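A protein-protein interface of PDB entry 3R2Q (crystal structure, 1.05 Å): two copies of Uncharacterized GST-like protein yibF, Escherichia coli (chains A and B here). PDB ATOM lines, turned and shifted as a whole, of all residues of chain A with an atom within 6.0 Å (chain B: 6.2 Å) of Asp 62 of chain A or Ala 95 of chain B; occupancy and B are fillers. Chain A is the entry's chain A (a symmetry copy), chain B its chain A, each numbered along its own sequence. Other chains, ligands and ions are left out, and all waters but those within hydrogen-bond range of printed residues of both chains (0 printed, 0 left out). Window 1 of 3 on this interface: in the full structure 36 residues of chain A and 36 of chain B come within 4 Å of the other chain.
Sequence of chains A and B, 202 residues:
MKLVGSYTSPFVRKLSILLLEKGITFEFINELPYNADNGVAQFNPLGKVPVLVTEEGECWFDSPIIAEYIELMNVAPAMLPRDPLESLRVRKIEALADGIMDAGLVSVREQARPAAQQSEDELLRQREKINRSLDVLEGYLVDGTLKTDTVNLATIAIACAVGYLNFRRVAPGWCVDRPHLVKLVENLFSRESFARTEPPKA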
ATOM      1  N   LEU A  15     -34.874 -20.417   2.733  1.00  0.00           N
ATOM      2  CA  LEU A  15     -34.879 -19.308   3.669  1.00  0.00           C
ATOM      3  C   LEU A  15     -36.284 -18.991   4.205  1.00  0.00           C
ATOM      4  O   LEU A  15     -36.426 -18.711   5.383  1.00  0.00           O
ATOM      5  CB  LEU A  15     -34.256 -18.080   3.029  1.00  0.00           C
ATOM      6  CG  LEU A  15     -32.847 -18.313   2.485  1.00  0.00           C
ATOM      7  CD1 LEU A  15     -32.388 -17.041   1.842  1.00  0.00           C
ATOM      8  CD2 LEU A  15     -31.886 -18.808   3.526  1.00  0.00           C
ATOM      9  N   LEU A  46     -25.572  -9.027  -8.535  1.00  0.00           N
ATOM     10  CA  LEU A  46     -25.556 -10.273  -9.297  1.00  0.00           C
ATOM     11  C   LEU A  46     -26.889 -10.561  -9.941  1.00  0.00           C
ATOM     12  O   LEU A  46     -26.960 -11.474 -10.771  1.00  0.00           O
ATOM     13  CB  LEU A  46     -25.138 -11.438  -8.410  1.00  0.00           C
ATOM     14  CG  LEU A  46     -23.748 -11.328  -7.788  1.00  0.00           C
ATOM     15  CD1 LEU A  46     -23.599 -12.394  -6.717  1.00  0.00           C
ATOM     16  CD2 LEU A  46     -22.666 -11.418  -8.833  1.00  0.00           C
ATOM     17  N   PRO A  50     -32.190 -15.605  -3.574  1.00  0.00           N
ATOM     18  CA  PRO A  50     -32.711 -14.654  -2.596  1.00  0.00           C
ATOM     19  C   PRO A  50     -31.749 -13.550  -2.234  1.00  0.00           C
ATOM     20  O   PRO A  50     -30.520 -13.648  -2.351  1.00  0.00           O
ATOM     21  CB  PRO A  50     -32.934 -15.533  -1.349  1.00  0.00           C
ATOM     22  CG  PRO A  50     -31.873 -16.614  -1.502  1.00  0.00           C
ATOM     23  CD  PRO A  50     -31.849 -16.900  -2.971  1.00  0.00           C
ATOM     24  N   TRP A  60     -28.122  -8.860   2.141  1.00  0.00           N
ATOM     25  CA  TRP A  60     -27.370 -10.103   2.330  1.00  0.00           C
ATOM     26  C   TRP A  60     -27.671 -11.067   1.209  1.00  0.00           C
ATOM     27  O   TRP A  60     -28.842 -11.266   0.843  1.00  0.00           O
ATOM     28  CB  TRP A  60     -27.720 -10.746   3.667  1.00  0.00           C
ATOM     29  CG  TRP A  60     -27.284  -9.919   4.835  1.00  0.00           C
ATOM     30  CD1 TRP A  60     -27.972  -8.916   5.478  1.00  0.00           C
ATOM     31  CD2 TRP A  60     -26.029 -10.027   5.508  1.00  0.00           C
ATOM     32  NE1 TRP A  60     -27.182  -8.422   6.498  1.00  0.00           N
ATOM     33  CE2 TRP A  60     -26.014  -9.098   6.518  1.00  0.00           C
ATOM     34  CE3 TRP A  60     -24.915 -10.843   5.337  1.00  0.00           C
ATOM     35  CZ2 TRP A  60     -24.903  -8.947   7.395  1.00  0.00           C
ATOM     36  CZ3 TRP A  60     -23.833 -10.685   6.193  1.00  0.00           C
ATOM     37  CH2 TRP A  60     -23.836  -9.775   7.182  1.00  0.00           C
ATOM     38  N   PHE A  61     -26.625 -11.737   0.709  1.00  0.00           N
ATOM     39  CA  PHE A  61     -26.695 -12.767  -0.311  1.00  0.00           C
ATOM     40  C   PHE A  61     -25.364 -13.500  -0.195  1.00  0.00           C
ATOM     41  O   PHE A  61     -24.409 -12.986   0.404  1.00  0.00           O
ATOM     42  CB  PHE A  61     -26.960 -12.176  -1.690  1.00  0.00           C
ATOM     43  CG  PHE A  61     -26.024 -11.050  -2.095  1.00  0.00           C
ATOM     44  CD1 PHE A  61     -24.806 -11.364  -2.689  1.00  0.00           C
ATOM     45  CD2 PHE A  61     -26.346  -9.732  -1.875  1.00  0.00           C
ATOM     46  CE1 PHE A  61     -23.925 -10.379  -3.063  1.00  0.00           C
ATOM     47  CE2 PHE A  61     -25.466  -8.754  -2.229  1.00  0.00           C
ATOM     48  CZ  PHE A  61     -24.237  -9.076  -2.783  1.00  0.00           C
ATOM     49  N   ASP A  62     -25.226 -14.668  -0.831  1.00  0.00           N
ATOM     50  CA  ASP A  62     -26.228 -15.528  -1.413  1.00  0.00           C
ATOM     51  C   ASP A  62     -26.914 -16.378  -0.349  1.00  0.00           C
ATOM     52  O   ASP A  62     -26.791 -16.121   0.855  1.00  0.00           O
ATOM     53  CB  ASP A  62     -25.636 -16.326  -2.567  1.00  0.00           C
ATOM     54  CG  ASP A  62     -24.547 -17.294  -2.183  1.00  0.00           C
ATOM     55  OD1 ASP A  62     -23.876 -17.074  -1.138  1.00  0.00           O
ATOM     56  OD2 ASP A  62     -24.348 -18.260  -2.962  1.00  0.00           O
ATOM     57  N   SER A  63     -27.714 -17.392  -0.744  1.00  0.00           N
ATOM     58  CA  SER A  63     -28.542 -18.083   0.192  1.00  0.00           C
ATOM     59  C   SER A  63     -27.821 -18.711   1.363  1.00  0.00           C
ATOM     60  O   SER A  63     -28.368 -18.639   2.484  1.00  0.00           O
ATOM     61  CB  SER A  63     -29.465 -19.100  -0.476  1.00  0.00           C
ATOM     62  OG  SER A  63     -28.831 -20.272  -0.920  1.00  0.00           O
ATOM     63  N   PRO A  64     -26.656 -19.353   1.250  1.00  0.00           N
ATOM     64  CA  PRO A  64     -26.021 -19.906   2.446  1.00  0.00           C
ATOM     65  C   PRO A  64     -25.646 -18.822   3.424  1.00  0.00           C
ATOM     66  O   PRO A  64     -25.721 -19.032   4.651  1.00  0.00           O
ATOM     67  CB  PRO A  64     -24.791 -20.680   1.897  1.00  0.00           C
ATOM     68  CG  PRO A  64     -24.866 -20.559   0.477  1.00  0.00           C
ATOM     69  CD  PRO A  64     -25.889 -19.705   0.022  1.00  0.00           C
ATOM     70  N   ILE A  65     -25.212 -17.660   2.955  1.00  0.00           N
ATOM     71  CA  ILE A  65     -24.849 -16.547   3.808  1.00  0.00           C
ATOM     72  C   ILE A  65     -26.064 -16.036   4.548  1.00  0.00           C
ATOM     73  O   ILE A  65     -26.011 -15.766   5.757  1.00  0.00           O
ATOM     74  CB  ILE A  65     -24.196 -15.418   2.970  1.00  0.00           C
ATOM     75  CG1 ILE A  65     -22.866 -15.870   2.352  1.00  0.00           C
ATOM     76  CG2 ILE A  65     -24.060 -14.134   3.767  1.00  0.00           C
ATOM     77  CD1 ILE A  65     -21.774 -16.125   3.375  1.00  0.00           C
ATOM     78  N   ILE A  66     -27.190 -15.904   3.835  1.00  0.00           N
ATOM     79  CA  ILE A  66     -28.416 -15.470   4.478  1.00  0.00           C
ATOM     80  C   ILE A  66     -28.841 -16.459   5.572  1.00  0.00           C
ATOM     81  O   ILE A  66     -29.260 -16.061   6.650  1.00  0.00           O
ATOM     82  CB  ILE A  66     -29.546 -15.258   3.481  1.00  0.00           C
ATOM     83  CG1 ILE A  66     -29.218 -14.210   2.423  1.00  0.00           C
ATOM     84  CG2 ILE A  66     -30.806 -14.884   4.226  1.00  0.00           C
ATOM     85  CD1 ILE A  66     -30.086 -14.279   1.198  1.00  0.00           C
ATOM     86  N   ALA A  67     -28.734 -17.742   5.285  1.00  0.00           N
ATOM     87  CA  ALA A  67     -29.126 -18.745   6.277  1.00  0.00           C
ATOM     88  C   ALA A  67     -28.249 -18.604   7.528  1.00  0.00           C
ATOM     89  O   ALA A  67     -28.760 -18.709   8.649  1.00  0.00           O
ATOM     90  CB  ALA A  67     -28.988 -20.146   5.681  1.00  0.00           C
ATOM     91  N   VAL B  90     -17.577 -10.205   5.769  1.00  0.00           N
ATOM     92  CA  VAL B  90     -16.478 -10.528   4.826  1.00  0.00           C
ATOM     93  C   VAL B  90     -16.907 -11.589   3.876  1.00  0.00           C
ATOM     94  O   VAL B  90     -16.612 -11.509   2.659  1.00  0.00           O
ATOM     95  CB  VAL B  90     -15.213 -10.922   5.607  1.00  0.00           C
ATOM     96  CG1 VAL B  90     -14.122 -11.331   4.630  1.00  0.00           C
ATOM     97  CG2 VAL B  90     -14.705  -9.763   6.438  1.00  0.00           C
ATOM     98  N   ARG B  91     -17.567 -12.641   4.360  1.00  0.00           N
ATOM     99  CA  ARG B  91     -18.040 -13.735   3.530  1.00  0.00           C
ATOM    100  C   ARG B  91     -19.165 -13.342   2.569  1.00  0.00           C
ATOM    101  O   ARG B  91     -19.281 -13.921   1.480  1.00  0.00           O
ATOM    102  CB  ARG B  91     -18.384 -14.983   4.382  1.00  0.00           C
ATOM    103  CG  ARG B  91     -17.100 -15.667   4.849  1.00  0.00           C
ATOM    104  CD  ARG B  91     -17.373 -16.826   5.785  1.00  0.00           C
ATOM    105  NE  ARG B  91     -17.692 -16.298   7.099  1.00  0.00           N
ATOM    106  CZ  ARG B  91     -18.449 -16.913   8.015  1.00  0.00           C
ATOM    107  NH1 ARG B  91     -19.085 -18.056   7.839  1.00  0.00           N
ATOM    108  NH2 ARG B  91     -18.574 -16.274   9.193  1.00  0.00           N
ATOM    109  N   LYS B  92     -19.950 -12.318   2.866  1.00  0.00           N
ATOM    110  CA  LYS B  92     -20.898 -11.758   1.908  1.00  0.00           C
ATOM    111  C   LYS B  92     -20.141 -11.160   0.744  1.00  0.00           C
ATOM    112  O   LYS B  92     -20.478 -11.354  -0.424  1.00  0.00           O
ATOM    113  CB  LYS B  92     -21.805 -10.747   2.622  1.00  0.00           C
ATOM    114  CG  LYS B  92     -23.064 -10.394   1.992  1.00  0.00           C
ATOM    115  CD  LYS B  92     -23.153  -9.731   0.699  1.00  0.00           C
ATOM    116  CE  LYS B  92     -22.699  -8.274   0.769  1.00  0.00           C
ATOM    117  NZ  LYS B  92     -23.417  -7.410   1.683  1.00  0.00           N
ATOM    118  N   ILE B  93     -19.060 -10.421   1.031  1.00  0.00           N
ATOM    119  CA  ILE B  93     -18.245  -9.848  -0.034  1.00  0.00           C
ATOM    120  C   ILE B  93     -17.561 -10.955  -0.830  1.00  0.00           C
ATOM    121  O   ILE B  93     -17.455 -10.876  -2.050  1.00  0.00           O
ATOM    122  CB  ILE B  93     -17.300  -8.771   0.494  1.00  0.00           C
ATOM    123  CG1 ILE B  93     -18.063  -7.668   1.214  1.00  0.00           C
ATOM    124  CG2 ILE B  93     -16.441  -8.205  -0.635  1.00  0.00           C
ATOM    125  CD1 ILE B  93     -17.168  -6.592   1.822  1.00  0.00           C
ATOM    126  N   GLU B  94     -17.104 -12.012  -0.155  1.00  0.00           N
ATOM    127  CA  GLU B  94     -16.593 -13.179  -0.874  1.00  0.00           C
ATOM    128  C   GLU B  94     -17.659 -13.731  -1.808  1.00  0.00           C
ATOM    129  O   GLU B  94     -17.343 -14.109  -2.935  1.00  0.00           O
ATOM    130  CB  GLU B  94     -16.134 -14.259   0.113  1.00  0.00           C
ATOM    131  CG  GLU B  94     -15.580 -15.491  -0.579  1.00  0.00           C
ATOM    132  CD  GLU B  94     -15.486 -16.726   0.304  1.00  0.00           C
ATOM    133  OE1 GLU B  94     -15.968 -16.601   1.498  1.00  0.00           O
ATOM    134  OE2 GLU B  94     -14.953 -17.755  -0.093  1.00  0.00           O
ATOM    135  N   ALA B  95     -18.899 -13.820  -1.366  1.00  0.00           N
ATOM    136  CA  ALA B  95     -19.985 -14.318  -2.216  1.00  0.00           C
ATOM    137  C   ALA B  95     -20.178 -13.429  -3.433  1.00  0.00           C
ATOM    138  O   ALA B  95     -20.452 -13.915  -4.525  1.00  0.00           O
ATOM    139  CB  ALA B  95     -21.280 -14.424  -1.423  1.00  0.00           C
ATOM    140  N   LEU B  96     -20.036 -12.116  -3.271  1.00  0.00           N
ATOM    141  CA  LEU B  96     -20.096 -11.200  -4.413  1.00  0.00           C
ATOM    142  C   LEU B  96     -18.991 -11.521  -5.412  1.00  0.00           C
ATOM    143  O   LEU B  96     -19.224 -11.625  -6.611  1.00  0.00           O
ATOM    144  CB  LEU B  96     -20.049  -9.756  -3.930  1.00  0.00           C
ATOM    145  CG  LEU B  96     -20.134  -8.715  -5.020  1.00  0.00           C
ATOM    146  CD1 LEU B  96     -21.328  -8.915  -5.936  1.00  0.00           C
ATOM    147  CD2 LEU B  96     -20.167  -7.312  -4.445  1.00  0.00           C
ATOM    148  N   ALA B  97     -17.744 -11.646  -4.901  1.00  0.00           N
ATOM    149  CA  ALA B  97     -16.635 -11.974  -5.785  1.00  0.00           C
ATOM    150  C   ALA B  97     -16.826 -13.316  -6.466  1.00  0.00           C
ATOM    151  O   ALA B  97     -16.549 -13.466  -7.666  1.00  0.00           O
ATOM    152  CB  ALA B  97     -15.348 -11.977  -4.973  1.00  0.00           C
ATOM    153  N   ASP B  98     -17.300 -14.322  -5.713  1.00  0.00           N
ATOM    154  CA  ASP B  98     -17.580 -15.605  -6.284  1.00  0.00           C
ATOM    155  C   ASP B  98     -18.651 -15.499  -7.369  1.00  0.00           C
ATOM    156  O   ASP B  98     -18.595 -16.233  -8.362  1.00  0.00           O
ATOM    157  CB  ASP B  98     -18.044 -16.576  -5.223  1.00  0.00           C
ATOM    158  CG  ASP B  98     -16.945 -17.047  -4.269  1.00  0.00           C
ATOM    159  OD1 ASP B  98     -15.765 -16.830  -4.490  1.00  0.00           O
ATOM    160  OD2 ASP B  98     -17.317 -17.729  -3.258  1.00  0.00           O
ATOM    161  N   GLY B  99     -19.629 -14.613  -7.192  1.00  0.00           N
ATOM    162  CA  GLY B  99     -20.615 -14.377  -8.212  1.00  0.00           C
ATOM    163  C   GLY B  99     -20.065 -13.743  -9.453  1.00  0.00           C
ATOM    164  O   GLY B  99     -20.553 -14.025 -10.571  1.00  0.00           O
ATOM    165  N   ILE B 100     -19.067 -12.886  -9.329  1.00  0.00           N
ATOM    166  CA  ILE B 100     -18.361 -12.387 -10.504  1.00  0.00           C
ATOM    167  C   ILE B 100     -17.685 -13.504 -11.237  1.00  0.00           C
ATOM    168  O   ILE B 100     -17.725 -13.615 -12.465  1.00  0.00           O
ATOM    169  CB  ILE B 100     -17.380 -11.240 -10.126  1.00  0.00           C
ATOM    170  CG1 ILE B 100     -18.153 -10.025  -9.576  1.00  0.00           C
ATOM    171  CG2 ILE B 100     -16.504 -10.847 -11.292  1.00  0.00           C
ATOM    172  CD1 ILE B 100     -17.324  -8.992  -8.892  1.00  0.00           C
ATOM    173  N   ASP B 102     -18.612 -16.630 -11.156  1.00  0.00           N
ATOM    174  CA  ASP B 102     -19.685 -17.413 -11.752  1.00  0.00           C
ATOM    175  C   ASP B 102     -20.092 -16.825 -13.111  1.00  0.00           C
ATOM    176  O   ASP B 102     -20.281 -17.555 -14.085  1.00  0.00           O
ATOM    177  CB  ASP B 102     -20.897 -17.490 -10.844  1.00  0.00           C
ATOM    178  CG  ASP B 102     -20.920 -18.225  -9.539  1.00  0.00           C
ATOM    179  OD1 ASP B 102     -20.125 -19.172  -9.412  1.00  0.00           O
ATOM    180  OD2 ASP B 102     -21.724 -17.921  -8.631  1.00  0.00           O
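Hydrophobic or aromatic side chains of chain B that line the printed part of chain A: Ala 95 and Leu 96.
Of the 11 printed residues of chain A, 5 touch a printed residue of chain B.
Hydrophobic or aromatic side chains of chain A that line the printed part of chain B: Leu 46, Trp 60, Phe 61 and Ile 65.
Asp 62 of chain A touches just one residue of chain B: Ala 95.
Ala 95 of chain B touches just these residues of chain A: Phe 61 (3.9 Å) and Asp 62 (3.7 Å).
Of the printed residues of chain B, Trp 60 of chain A touches Lys 92.
Printed residues of chain A within 4 Å of Arg 91 of chain B: Ile 65.
Printed residues of chain A within 4 Å of Lys 92 of chain B: Trp 60 (3.8 Å) and Phe 61 (3.3 Å).
Printed residues of chain A within 4 Å of Ile 100 of chain B: Leu 46 (3.9 Å).
Glu 94 of chain B touches none of the printed residues of chain A.
Ile 66 of chain A touches none of the printed residues of chain B.
The nearest printed residue of chain B that does not touch Phe 61 of chain A is Leu 96 of chain B (4.02 Å).
No position is printed for both chains.
Of the 8 pairs that touch across the chains among the printed residues, none has its exchanged pair printed and touching as well.
Among the printed residues, merely in contact across the chains: Phe 61 of chain A with Lys 92 of chain B (3.3 Å), Leu 46 of chain A with Gly 99 of chain B (3.5 Å), Ile 65 of chain A with Arg 91 of chain B (3.7 Å), Asp 62 of chain A with Ala 95 of chain B (3.7 Å), Trp 60 of chain A with Lys 92 of chain B (3.8 Å), Leu 46 of chain A with Leu 96 of chain B (3.9 Å), Phe 61 of chain A with Ala 95 of chain B (3.9 Å) and Leu 46 of chain A with Ile 100 of chain B (3.9 Å).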
